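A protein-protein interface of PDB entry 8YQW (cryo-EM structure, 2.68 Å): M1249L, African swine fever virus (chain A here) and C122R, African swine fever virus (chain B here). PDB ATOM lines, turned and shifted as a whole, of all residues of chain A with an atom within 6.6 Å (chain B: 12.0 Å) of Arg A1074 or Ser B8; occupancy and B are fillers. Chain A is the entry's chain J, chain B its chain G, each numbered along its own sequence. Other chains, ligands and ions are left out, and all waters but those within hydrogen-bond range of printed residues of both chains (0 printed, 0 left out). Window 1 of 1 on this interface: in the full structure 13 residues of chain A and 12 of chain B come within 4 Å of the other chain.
O of Ala B6 sits at hydrogen-bond distance from NE2 of His A1123 (2.5 Å). The backbone carbonyl oxygen (O) of Cys B7 is in hydrogen-bond range of the guanidinium group (NH1) of Arg A1074. OG of Ser B8 sits at hydrogen-bond distance from ND1 of His A1123, 3.4 Å away.
The backbone NH (N) of Ala B6 sits close to the side-chain sulfur (SG) of Cys B4, at 3.5 Å. The side-chain carboxylate of Asp A1070 lies within salt-bridge range of the guanidinium group of Arg A1074 (2.5 Å).
Among the printed residues, pairs that only touch across the chains: His A1123 with Lys B5, Arg A1074 with Ser B8, Tyr A1078 with Cys B26, Tyr A1078 with Ser B25, Leu A1077 with Ala B6 and Tyr A1078 with Cys B7.
No residue of chain B comes within 4 Å of Asp A1070. No residue of chain B comes within 4 Å of Ala A1072. Printed residues of chain B within 4 Å of Arg A1074: Cys B7 (3.2 Å) and Ser B8 (3.3 Å). No residue of chain B comes within 4 Å of Ile A1075. Of chain B, only Ala B6 (3.8 Å) comes within 4 Å of Leu A1077. Of the printed residues of chain B, Tyr A1078 touches Cys B7, Ser B25 and Cys B26. His A1123 touches just these residues of chain B: Lys B5 (3.2 Å), Ala B6 (2.5 Å) and Ser B8 (3.4 Å). Printed residues of chain A within 4 Å of Lys B5: His A1123 (3.2 Å). Of the printed residues of chain A, Cys B7 touches Arg A1074 and Tyr A1078. Ser B8 touches just these residues of chain A: Arg A1074 and His A1123. Of the printed residues of chain A, Ser B25 touches Tyr A1078 (3.5 Å). Of the printed residues of chain A, Cys B26 touches Tyr A1078 (3.5 Å). The nearest residue of chain B that does not touch Arg A1074 is Ala B6 (5.2 Å). The nearest residue of chain A that does not touch Ser B8 is Lys A1127 (5.2 Å). The nearest printed residue of chain A that does not touch Lys B5 is Leu A1077 (6.2 Å).
Of the 21 printed residues of chain B, 6 touch a printed residue of chain A. Of the 17 printed residues of chain A, 4 touch a printed residue of chain B. Among the printed residues, 9 pairs touch across the chains.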
ATOM      1  N   MET A1067     -15.778 -15.099  17.978  1.00  0.00           N
ATOM      2  CA  MET A1067     -17.230 -15.046  18.112  1.00  0.00           C
ATOM      3  C   MET A1067     -17.919 -15.031  16.754  1.00  0.00           C
ATOM      4  O   MET A1067     -19.040 -15.533  16.625  1.00  0.00           O
ATOM      5  CB  MET A1067     -17.634 -13.818  18.927  1.00  0.00           C
ATOM      6  CG  MET A1067     -17.319 -13.914  20.413  1.00  0.00           C
ATOM      7  SD  MET A1067     -18.397 -15.053  21.296  1.00  0.00           S
ATOM      8  CE  MET A1067     -17.309 -16.456  21.520  1.00  0.00           C
ATOM      9  N   VAL A1069     -16.925 -16.561  13.844  1.00  0.00           N
ATOM     10  CA  VAL A1069     -16.967 -17.890  13.243  1.00  0.00           C
ATOM     11  C   VAL A1069     -17.906 -18.797  14.025  1.00  0.00           C
ATOM     12  O   VAL A1069     -18.628 -19.616  13.445  1.00  0.00           O
ATOM     13  CB  VAL A1069     -15.553 -18.486  13.148  1.00  0.00           C
ATOM     14  CG1 VAL A1069     -15.587 -19.795  12.377  1.00  0.00           C
ATOM     15  CG2 VAL A1069     -14.607 -17.503  12.502  1.00  0.00           C
ATOM     16  N   ASP A1070     -17.909 -18.670  15.354  1.00  0.00           N
ATOM     17  CA  ASP A1070     -18.838 -19.442  16.171  1.00  0.00           C
ATOM     18  C   ASP A1070     -20.281 -19.077  15.852  1.00  0.00           C
ATOM     19  O   ASP A1070     -21.164 -19.941  15.856  1.00  0.00           O
ATOM     20  CB  ASP A1070     -18.542 -19.219  17.653  1.00  0.00           C
ATOM     21  CG  ASP A1070     -19.597 -19.821  18.554  1.00  0.00           C
ATOM     22  OD1 ASP A1070     -19.740 -21.059  18.551  1.00  0.00           O
ATOM     23  OD2 ASP A1070     -20.283 -19.058  19.266  1.00  0.00           O
ATOM     24  N   SER A1071     -20.540 -17.797  15.581  1.00  0.00           N
ATOM     25  CA  SER A1071     -21.873 -17.387  15.157  1.00  0.00           C
ATOM     26  C   SER A1071     -22.248 -18.031  13.829  1.00  0.00           C
ATOM     27  O   SER A1071     -23.407 -18.407  13.619  1.00  0.00           O
ATOM     28  CB  SER A1071     -21.943 -15.864  15.055  1.00  0.00           C
ATOM     29  OG  SER A1071     -23.221 -15.442  14.620  1.00  0.00           O
ATOM     30  N   ALA A1072     -21.280 -18.163  12.920  1.00  0.00           N
ATOM     31  CA  ALA A1072     -21.544 -18.822  11.646  1.00  0.00           C
ATOM     32  C   ALA A1072     -21.907 -20.288  11.843  1.00  0.00           C
ATOM     33  O   ALA A1072     -22.770 -20.822  11.137  1.00  0.00           O
ATOM     34  CB  ALA A1072     -20.332 -18.691  10.725  1.00  0.00           C
ATOM     35  N   VAL A1073     -21.248 -20.961  12.788  1.00  0.00           N
ATOM     36  CA  VAL A1073     -21.523 -22.376  13.019  1.00  0.00           C
ATOM     37  C   VAL A1073     -22.947 -22.575  13.516  1.00  0.00           C
ATOM     38  O   VAL A1073     -23.671 -23.452  13.030  1.00  0.00           O
ATOM     39  CB  VAL A1073     -20.496 -22.967  14.002  1.00  0.00           C
ATOM     40  CG1 VAL A1073     -20.912 -24.362  14.420  1.00  0.00           C
ATOM     41  CG2 VAL A1073     -19.117 -22.993  13.375  1.00  0.00           C
ATOM     42  N   ARG A1074     -23.381 -21.764  14.483  1.00  0.00           N
ATOM     43  CA  ARG A1074     -24.664 -22.022  15.123  1.00  0.00           C
ATOM     44  C   ARG A1074     -25.855 -21.637  14.258  1.00  0.00           C
ATOM     45  O   ARG A1074     -26.970 -22.077  14.547  1.00  0.00           O
ATOM     46  CB  ARG A1074     -24.760 -21.300  16.469  1.00  0.00           C
ATOM     47  CG  ARG A1074     -25.151 -19.839  16.390  1.00  0.00           C
ATOM     48  CD  ARG A1074     -25.302 -19.252  17.786  1.00  0.00           C
ATOM     49  NE  ARG A1074     -24.029 -19.196  18.496  1.00  0.00           N
ATOM     50  CZ  ARG A1074     -23.693 -20.006  19.489  1.00  0.00           C
ATOM     51  NH1 ARG A1074     -24.512 -20.950  19.919  1.00  0.00           N
ATOM     52  NH2 ARG A1074     -22.501 -19.868  20.063  1.00  0.00           N
ATOM     53  N   ILE A1075     -25.660 -20.830  13.213  1.00  0.00           N
ATOM     54  CA  ILE A1075     -26.755 -20.618  12.271  1.00  0.00           C
ATOM     55  C   ILE A1075     -26.851 -21.767  11.281  1.00  0.00           C
ATOM     56  O   ILE A1075     -27.921 -21.990  10.704  1.00  0.00           O
ATOM     57  CB  ILE A1075     -26.630 -19.279  11.524  1.00  0.00           C
ATOM     58  CG1 ILE A1075     -25.474 -19.301  10.532  1.00  0.00           C
ATOM     59  CG2 ILE A1075     -26.446 -18.136  12.498  1.00  0.00           C
ATOM     60  CD1 ILE A1075     -25.428 -18.075   9.660  1.00  0.00           C
ATOM     61  N   PHE A1076     -25.760 -22.501  11.065  1.00  0.00           N
ATOM     62  CA  PHE A1076     -25.849 -23.755  10.327  1.00  0.00           C
ATOM     63  C   PHE A1076     -26.568 -24.817  11.147  1.00  0.00           C
ATOM     64  O   PHE A1076     -27.382 -25.577  10.611  1.00  0.00           O
ATOM     65  CB  PHE A1076     -24.452 -24.232   9.932  1.00  0.00           C
ATOM     66  CG  PHE A1076     -24.451 -25.383   8.967  1.00  0.00           C
ATOM     67  CD1 PHE A1076     -24.542 -26.687   9.423  1.00  0.00           C
ATOM     68  CD2 PHE A1076     -24.362 -25.161   7.606  1.00  0.00           C
ATOM     69  CE1 PHE A1076     -24.542 -27.744   8.539  1.00  0.00           C
ATOM     70  CE2 PHE A1076     -24.362 -26.215   6.718  1.00  0.00           C
ATOM     71  CZ  PHE A1076     -24.452 -27.508   7.185  1.00  0.00           C
ATOM     72  N   LEU A1077     -26.278 -24.885  12.446  1.00  0.00           N
ATOM     73  CA  LEU A1077     -26.946 -25.857  13.304  1.00  0.00           C
ATOM     74  C   LEU A1077     -28.393 -25.464  13.563  1.00  0.00           C
ATOM     75  O   LEU A1077     -29.278 -26.326  13.601  1.00  0.00           O
ATOM     76  CB  LEU A1077     -26.183 -26.002  14.618  1.00  0.00           C
ATOM     77  CG  LEU A1077     -24.697 -26.323  14.479  1.00  0.00           C
ATOM     78  CD1 LEU A1077     -23.969 -26.063  15.783  1.00  0.00           C
ATOM     79  CD2 LEU A1077     -24.504 -27.758  14.025  1.00  0.00           C
ATOM     80  N   TYR A1078     -28.656 -24.169  13.747  1.00  0.00           N
ATOM     81  CA  TYR A1078     -30.026 -23.719  13.968  1.00  0.00           C
ATOM     82  C   TYR A1078     -30.901 -24.001  12.756  1.00  0.00           C
ATOM     83  O   TYR A1078     -32.038 -24.469  12.895  1.00  0.00           O
ATOM     84  CB  TYR A1078     -30.042 -22.229  14.307  1.00  0.00           C
ATOM     85  CG  TYR A1078     -31.425 -21.626  14.405  1.00  0.00           C
ATOM     86  CD1 TYR A1078     -32.129 -21.647  15.600  1.00  0.00           C
ATOM     87  CD2 TYR A1078     -32.019 -21.020  13.306  1.00  0.00           C
ATOM     88  CE1 TYR A1078     -33.389 -21.092  15.692  1.00  0.00           C
ATOM     89  CE2 TYR A1078     -33.275 -20.466  13.389  1.00  0.00           C
ATOM     90  CZ  TYR A1078     -33.956 -20.502  14.584  1.00  0.00           C
ATOM     91  OH  TYR A1078     -35.209 -19.946  14.667  1.00  0.00           O
ATOM     92  N   ASN A1079     -30.387 -23.729  11.555  1.00  0.00           N
ATOM     93  CA  ASN A1079     -31.174 -23.962  10.352  1.00  0.00           C
ATOM     94  C   ASN A1079     -31.276 -25.445  10.024  1.00  0.00           C
ATOM     95  O   ASN A1079     -32.258 -25.874   9.410  1.00  0.00           O
ATOM     96  CB  ASN A1079     -30.570 -23.198   9.177  1.00  0.00           C
ATOM     97  CG  ASN A1079     -30.912 -21.722   9.204  1.00  0.00           C
ATOM     98  OD1 ASN A1079     -31.980 -21.330   9.674  1.00  0.00           O
ATOM     99  ND2 ASN A1079     -30.007 -20.893   8.695  1.00  0.00           N
ATOM    100  N   TYR A1122     -19.673 -29.785  19.743  1.00  0.00           N
ATOM    101  CA  TYR A1122     -19.074 -28.529  19.305  1.00  0.00           C
ATOM    102  C   TYR A1122     -19.047 -27.497  20.424  1.00  0.00           C
ATOM    103  O   TYR A1122     -17.992 -26.936  20.734  1.00  0.00           O
ATOM    104  CB  TYR A1122     -19.823 -27.962  18.102  1.00  0.00           C
ATOM    105  CG  TYR A1122     -19.480 -26.514  17.849  1.00  0.00           C
ATOM    106  CD1 TYR A1122     -18.219 -26.151  17.400  1.00  0.00           C
ATOM    107  CD2 TYR A1122     -20.404 -25.509  18.084  1.00  0.00           C
ATOM    108  CE1 TYR A1122     -17.895 -24.829  17.179  1.00  0.00           C
ATOM    109  CE2 TYR A1122     -20.087 -24.183  17.868  1.00  0.00           C
ATOM    110  CZ  TYR A1122     -18.832 -23.851  17.415  1.00  0.00           C
ATOM    111  OH  TYR A1122     -18.515 -22.532  17.196  1.00  0.00           O
ATOM    112  N   HIS A1123     -20.204 -27.230  21.034  1.00  0.00           N
ATOM    113  CA  HIS A1123     -20.303 -26.140  22.000  1.00  0.00           C
ATOM    114  C   HIS A1123     -19.392 -26.368  23.197  1.00  0.00           C
ATOM    115  O   HIS A1123     -18.761 -25.429  23.693  1.00  0.00           O
ATOM    116  CB  HIS A1123     -21.754 -25.976  22.455  1.00  0.00           C
ATOM    117  CG  HIS A1123     -22.699 -25.619  21.350  1.00  0.00           C
ATOM    118  ND1 HIS A1123     -22.606 -24.441  20.643  1.00  0.00           N
ATOM    119  CD2 HIS A1123     -23.759 -26.285  20.835  1.00  0.00           C
ATOM    120  CE1 HIS A1123     -23.567 -24.396  19.737  1.00  0.00           C
ATOM    121  NE2 HIS A1123     -24.280 -25.504  19.833  1.00  0.00           N
ATOM    122  N   PHE A1126     -15.663 -25.821  21.935  1.00  0.00           N
ATOM    123  CA  PHE A1126     -15.311 -24.453  21.572  1.00  0.00           C
ATOM    124  C   PHE A1126     -15.022 -23.607  22.804  1.00  0.00           C
ATOM    125  O   PHE A1126     -14.076 -22.812  22.808  1.00  0.00           O
ATOM    126  CB  PHE A1126     -16.422 -23.817  20.741  1.00  0.00           C
ATOM    127  CG  PHE A1126     -16.153 -22.387  20.375  1.00  0.00           C
ATOM    128  CD1 PHE A1126     -15.241 -22.072  19.384  1.00  0.00           C
ATOM    129  CD2 PHE A1126     -16.806 -21.356  21.027  1.00  0.00           C
ATOM    130  CE1 PHE A1126     -14.989 -20.757  19.049  1.00  0.00           C
ATOM    131  CE2 PHE A1126     -16.559 -20.043  20.697  1.00  0.00           C
ATOM    132  CZ  PHE A1126     -15.649 -19.743  19.706  1.00  0.00           C
ATOM    133  N   LYS A1127     -15.826 -23.760  23.858  1.00  0.00           N
ATOM    134  CA  LYS A1127     -15.604 -22.975  25.067  1.00  0.00           C
ATOM    135  C   LYS A1127     -14.302 -23.362  25.754  1.00  0.00           C
ATOM    136  O   LYS A1127     -13.693 -22.534  26.439  1.00  0.00           O
ATOM    137  CB  LYS A1127     -16.782 -23.135  26.023  1.00  0.00           C
ATOM    138  CG  LYS A1127     -18.123 -22.781  25.408  1.00  0.00           C
ATOM    139  CD  LYS A1127     -18.148 -21.350  24.900  1.00  0.00           C
ATOM    140  CE  LYS A1127     -19.546 -20.949  24.459  1.00  0.00           C
ATOM    141  NZ  LYS A1127     -19.997 -21.716  23.264  1.00  0.00           N
ATOM    142  N   LEU A1145     -17.368 -26.455  10.730  1.00  0.00           N
ATOM    143  CA  LEU A1145     -18.363 -26.064   9.737  1.00  0.00           C
ATOM    144  C   LEU A1145     -18.182 -26.841   8.440  1.00  0.00           C
ATOM    145  O   LEU A1145     -19.161 -27.170   7.763  1.00  0.00           O
ATOM    146  CB  LEU A1145     -18.277 -24.561   9.478  1.00  0.00           C
ATOM    147  CG  LEU A1145     -19.444 -23.935   8.719  1.00  0.00           C
ATOM    148  CD1 LEU A1145     -20.759 -24.251   9.415  1.00  0.00           C
ATOM    149  CD2 LEU A1145     -19.247 -22.434   8.597  1.00  0.00           C
ATOM    150  N   MET B   1     -32.299 -21.198  33.498  1.00  0.00           N
ATOM    151  CA  MET B   1     -33.001 -21.524  32.266  1.00  0.00           C
ATOM    152  C   MET B   1     -32.573 -22.891  31.749  1.00  0.00           C
ATOM    153  O   MET B   1     -31.784 -23.588  32.386  1.00  0.00           O
ATOM    154  CB  MET B   1     -32.732 -20.471  31.192  1.00  0.00           C
ATOM    155  CG  MET B   1     -31.353 -20.586  30.552  1.00  0.00           C
ATOM    156  SD  MET B   1     -29.981 -20.058  31.591  1.00  0.00           S
ATOM    157  CE  MET B   1     -30.179 -18.286  31.498  1.00  0.00           C
ATOM    158  N   LYS B   2     -33.100 -23.270  30.589  1.00  0.00           N
ATOM    159  CA  LYS B   2     -32.601 -24.403  29.827  1.00  0.00           C
ATOM    160  C   LYS B   2     -31.991 -23.887  28.533  1.00  0.00           C
ATOM    161  O   LYS B   2     -32.585 -23.040  27.857  1.00  0.00           O
ATOM    162  CB  LYS B   2     -33.709 -25.414  29.533  1.00  0.00           C
ATOM    163  CG  LYS B   2     -33.238 -26.624  28.749  1.00  0.00           C
ATOM    164  CD  LYS B   2     -32.457 -27.588  29.621  1.00  0.00           C
ATOM    165  CE  LYS B   2     -33.376 -28.569  30.322  1.00  0.00           C
ATOM    166  NZ  LYS B   2     -32.609 -29.644  31.008  1.00  0.00           N
ATOM    167  N   ILE B   3     -30.808 -24.391  28.196  1.00  0.00           N
ATOM    168  CA  ILE B   3     -30.059 -23.949  27.027  1.00  0.00           C
ATOM    169  C   ILE B   3     -30.115 -25.049  25.979  1.00  0.00           C
ATOM    170  O   ILE B   3     -29.773 -26.204  26.260  1.00  0.00           O
ATOM    171  CB  ILE B   3     -28.606 -23.603  27.392  1.00  0.00           C
ATOM    172  CG1 ILE B   3     -28.548 -22.271  28.145  1.00  0.00           C
ATOM    173  CG2 ILE B   3     -27.737 -23.555  26.154  1.00  0.00           C
ATOM    174  CD1 ILE B   3     -29.143 -21.113  27.387  1.00  0.00           C
ATOM    175  N   CYS B   4     -30.556 -24.691  24.773  1.00  0.00           N
ATOM    176  CA  CYS B   4     -30.647 -25.654  23.686  1.00  0.00           C
ATOM    177  C   CYS B   4     -29.273 -26.224  23.361  1.00  0.00           C
ATOM    178  O   CYS B   4     -28.296 -25.487  23.216  1.00  0.00           O
ATOM    179  CB  CYS B   4     -31.250 -24.986  22.449  1.00  0.00           C
ATOM    180  SG  CYS B   4     -31.625 -26.098  21.080  1.00  0.00           S
ATOM    181  N   LYS B   5     -29.198 -27.551  23.247  1.00  0.00           N
ATOM    182  CA  LYS B   5     -27.917 -28.178  22.947  1.00  0.00           C
ATOM    183  C   LYS B   5     -27.504 -27.954  21.500  1.00  0.00           C
ATOM    184  O   LYS B   5     -26.331 -28.135  21.157  1.00  0.00           O
ATOM    185  CB  LYS B   5     -27.972 -29.672  23.262  1.00  0.00           C
ATOM    186  CG  LYS B   5     -28.184 -29.997  24.735  1.00  0.00           C
ATOM    187  CD  LYS B   5     -26.944 -29.698  25.570  1.00  0.00           C
ATOM    188  CE  LYS B   5     -27.091 -28.398  26.356  1.00  0.00           C
ATOM    189  NZ  LYS B   5     -25.929 -28.136  27.245  1.00  0.00           N
ATOM    190  N   ALA B   6     -28.446 -27.567  20.640  1.00  0.00           N
ATOM    191  CA  ALA B   6     -28.126 -27.317  19.240  1.00  0.00           C
ATOM    192  C   ALA B   6     -27.598 -25.902  19.025  1.00  0.00           C
ATOM    193  O   ALA B   6     -26.459 -25.712  18.590  1.00  0.00           O
ATOM    194  CB  ALA B   6     -29.361 -27.567  18.375  1.00  0.00           C
ATOM    195  N   CYS B   7     -28.416 -24.895  19.329  1.00  0.00           N
ATOM    196  CA  CYS B   7     -28.096 -23.509  19.015  1.00  0.00           C
ATOM    197  C   CYS B   7     -27.802 -22.661  20.246  1.00  0.00           C
ATOM    198  O   CYS B   7     -27.699 -21.437  20.126  1.00  0.00           O
ATOM    199  CB  CYS B   7     -29.235 -22.882  18.210  1.00  0.00           C
ATOM    200  SG  CYS B   7     -30.851 -22.976  19.005  1.00  0.00           S
ATOM    201  N   SER B   8     -27.669 -23.278  21.422  1.00  0.00           N
ATOM    202  CA  SER B   8     -27.352 -22.573  22.668  1.00  0.00           C
ATOM    203  C   SER B   8     -28.343 -21.454  22.966  1.00  0.00           C
ATOM    204  O   SER B   8     -27.989 -20.448  23.584  1.00  0.00           O
ATOM    205  CB  SER B   8     -25.923 -22.025  22.652  1.00  0.00           C
ATOM    206  OG  SER B   8     -24.973 -23.072  22.740  1.00  0.00           O
ATOM    207  N   SER B   9     -29.589 -21.619  22.541  1.00  0.00           N
ATOM    208  CA  SER B   9     -30.626 -20.624  22.759  1.00  0.00           C
ATOM    209  C   SER B   9     -31.364 -20.907  24.062  1.00  0.00           C
ATOM    210  O   SER B   9     -31.284 -21.995  24.632  1.00  0.00           O
ATOM    211  CB  SER B   9     -31.604 -20.601  21.582  1.00  0.00           C
ATOM    212  OG  SER B   9     -32.617 -19.634  21.780  1.00  0.00           O
ATOM    213  N   CYS B  10     -32.091 -19.898  24.533  1.00  0.00           N
ATOM    214  CA  CYS B  10     -32.876 -20.007  25.758  1.00  0.00           C
ATOM    215  C   CYS B  10     -34.242 -20.584  25.408  1.00  0.00           C
ATOM    216  O   CYS B  10     -35.048 -19.931  24.737  1.00  0.00           O
ATOM    217  CB  CYS B  10     -33.004 -18.648  26.437  1.00  0.00           C
ATOM    218  SG  CYS B  10     -34.046 -18.659  27.901  1.00  0.00           S
ATOM    219  N   MET B  11     -34.503 -21.804  25.863  1.00  0.00           N
ATOM    220  CA  MET B  11     -35.728 -22.506  25.511  1.00  0.00           C
ATOM    221  C   MET B  11     -36.912 -21.977  26.313  1.00  0.00           C
ATOM    222  O   MET B  11     -36.755 -21.385  27.383  1.00  0.00           O
ATOM    223  CB  MET B  11     -35.564 -24.006  25.748  1.00  0.00           C
ATOM    224  CG  MET B  11     -34.466 -24.642  24.919  1.00  0.00           C
ATOM    225  SD  MET B  11     -34.238 -26.387  25.296  1.00  0.00           S
ATOM    226  CE  MET B  11     -34.702 -27.132  23.738  1.00  0.00           C
ATOM    227  N   VAL B  12     -38.112 -22.205  25.780  1.00  0.00           N
ATOM    228  CA  VAL B  12     -39.349 -21.775  26.423  1.00  0.00           C
ATOM    229  C   VAL B  12     -39.951 -22.956  27.170  1.00  0.00           C
ATOM    230  O   VAL B  12     -40.038 -24.064  26.630  1.00  0.00           O
ATOM    231  CB  VAL B  12     -40.336 -21.210  25.389  1.00  0.00           C
ATOM    232  CG1 VAL B  12     -41.649 -20.839  26.054  1.00  0.00           C
ATOM    233  CG2 VAL B  12     -39.736 -20.006  24.687  1.00  0.00           C
ATOM    234  N   PHE B  22     -39.223 -28.176  27.673  1.00  0.00           N
ATOM    235  CA  PHE B  22     -38.543 -27.011  27.129  1.00  0.00           C
ATOM    236  C   PHE B  22     -38.500 -27.136  25.613  1.00  0.00           C
ATOM    237  O   PHE B  22     -37.871 -28.055  25.078  1.00  0.00           O
ATOM    238  CB  PHE B  22     -37.130 -26.890  27.695  1.00  0.00           C
ATOM    239  CG  PHE B  22     -37.088 -26.626  29.168  1.00  0.00           C
ATOM    240  CD1 PHE B  22     -37.296 -25.351  29.661  1.00  0.00           C
ATOM    241  CD2 PHE B  22     -36.829 -27.650  30.058  1.00  0.00           C
ATOM    242  CE1 PHE B  22     -37.254 -25.106  31.016  1.00  0.00           C
ATOM    243  CE2 PHE B  22     -36.784 -27.409  31.412  1.00  0.00           C
ATOM    244  CZ  PHE B  22     -36.997 -26.136  31.892  1.00  0.00           C
ATOM    245  N   ARG B  23     -39.165 -26.216  24.927  1.00  0.00           N
ATOM    246  CA  ARG B  23     -39.212 -26.186  23.474  1.00  0.00           C
ATOM    247  C   ARG B  23     -38.469 -24.955  22.977  1.00  0.00           C
ATOM    248  O   ARG B  23     -38.727 -23.838  23.440  1.00  0.00           O
ATOM    249  CB  ARG B  23     -40.658 -26.180  22.976  1.00  0.00           C
ATOM    250  CG  ARG B  23     -40.819 -26.593  21.524  1.00  0.00           C
ATOM    251  CD  ARG B  23     -42.278 -26.810  21.169  1.00  0.00           C
ATOM    252  NE  ARG B  23     -42.839 -27.968  21.857  1.00  0.00           N
ATOM    253  CZ  ARG B  23     -43.818 -27.911  22.750  1.00  0.00           C
ATOM    254  NH1 ARG B  23     -44.375 -26.761  23.094  1.00  0.00           N
ATOM    255  NH2 ARG B  23     -44.250 -29.036  23.311  1.00  0.00           N
ATOM    256  N   CYS B  24     -37.545 -25.163  22.048  1.00  0.00           N
ATOM    257  CA  CYS B  24     -36.773 -24.089  21.449  1.00  0.00           C
ATOM    258  C   CYS B  24     -37.445 -23.607  20.170  1.00  0.00           C
ATOM    259  O   CYS B  24     -38.388 -24.217  19.662  1.00  0.00           O
ATOM    260  CB  CYS B  24     -35.343 -24.555  21.163  1.00  0.00           C
ATOM    261  SG  CYS B  24     -34.216 -23.247  20.645  1.00  0.00           S
ATOM    262  N   SER B  25     -36.941 -22.491  19.644  1.00  0.00           N
ATOM    263  CA  SER B  25     -37.454 -21.950  18.394  1.00  0.00           C
ATOM    264  C   SER B  25     -36.896 -22.664  17.173  1.00  0.00           C
ATOM    265  O   SER B  25     -37.325 -22.368  16.053  1.00  0.00           O
ATOM    266  CB  SER B  25     -37.149 -20.453  18.299  1.00  0.00           C
ATOM    267  OG  SER B  25     -35.756 -20.221  18.191  1.00  0.00           O
ATOM    268  N   CYS B  26     -35.956 -23.588  17.359  1.00  0.00           N
ATOM    269  CA  CYS B  26     -35.413 -24.396  16.276  1.00  0.00           C
ATOM    270  C   CYS B  26     -36.058 -25.773  16.199  1.00  0.00           C
ATOM    271  O   CYS B  26     -35.575 -26.632  15.454  1.00  0.00           O
ATOM    272  CB  CYS B  26     -33.898 -24.536  16.429  1.00  0.00           C
ATOM    273  SG  CYS B  26     -33.359 -25.594  17.788  1.00  0.00           S
ATOM    274  N   GLY B  27     -37.130 -26.004  16.953  1.00  0.00           N
ATOM    275  CA  GLY B  27     -37.839 -27.260  16.929  1.00  0.00           C
ATOM    276  C   GLY B  27     -37.354 -28.288  17.927  1.00  0.00           C
ATOM    277  O   GLY B  27     -38.099 -29.223  18.242  1.00  0.00           O
ATOM    278  N   GLU B  28     -36.134 -28.143  18.435  1.00  0.00           N
ATOM    279  CA  GLU B  28     -35.620 -29.081  19.423  1.00  0.00           C
ATOM    280  C   GLU B  28     -36.395 -28.939  20.724  1.00  0.00           C
ATOM    281  O   GLU B  28     -36.632 -27.826  21.200  1.00  0.00           O
ATOM    282  CB  GLU B  28     -34.132 -28.838  19.658  1.00  0.00           C
ATOM    283  CG  GLU B  28     -33.560 -29.584  20.851  1.00  0.00           C
ATOM    284  CD  GLU B  28     -33.146 -30.999  20.508  1.00  0.00           C
ATOM    285  OE1 GLU B  28     -32.773 -31.245  19.343  1.00  0.00           O
ATOM    286  OE2 GLU B  28     -33.195 -31.866  21.406  1.00  0.00           O
ATOM    287  N   SER B  29     -36.802 -30.070  21.293  1.00  0.00           N
ATOM    288  CA  SER B  29     -37.537 -30.097  22.546  1.00  0.00           C
ATOM    289  C   SER B  29     -36.904 -31.112  23.482  1.00  0.00           C
ATOM    290  O   SER B  29     -36.503 -32.199  23.056  1.00  0.00           O
ATOM    291  CB  SER B  29     -39.012 -30.441  22.325  1.00  0.00           C
ATOM    292  OG  SER B  29     -39.169 -31.814  22.016  1.00  0.00           O
ATOM    293  N   VAL B  30     -36.812 -30.747  24.759  1.00  0.00           N
ATOM    294  CA  VAL B  30     -36.257 -31.604  25.796  1.00  0.00           C
ATOM    295  C   VAL B  30     -37.219 -31.564  26.978  1.00  0.00           C
ATOM    296  O   VAL B  30     -38.124 -30.734  27.037  1.00  0.00           O
ATOM    297  CB  VAL B  30     -34.834 -31.162  26.212  1.00  0.00           C
ATOM    298  CG1 VAL B  30     -34.876 -29.837  26.961  1.00  0.00           C
ATOM    299  CG2 VAL B  30     -34.110 -32.246  27.005  1.00  0.00           C
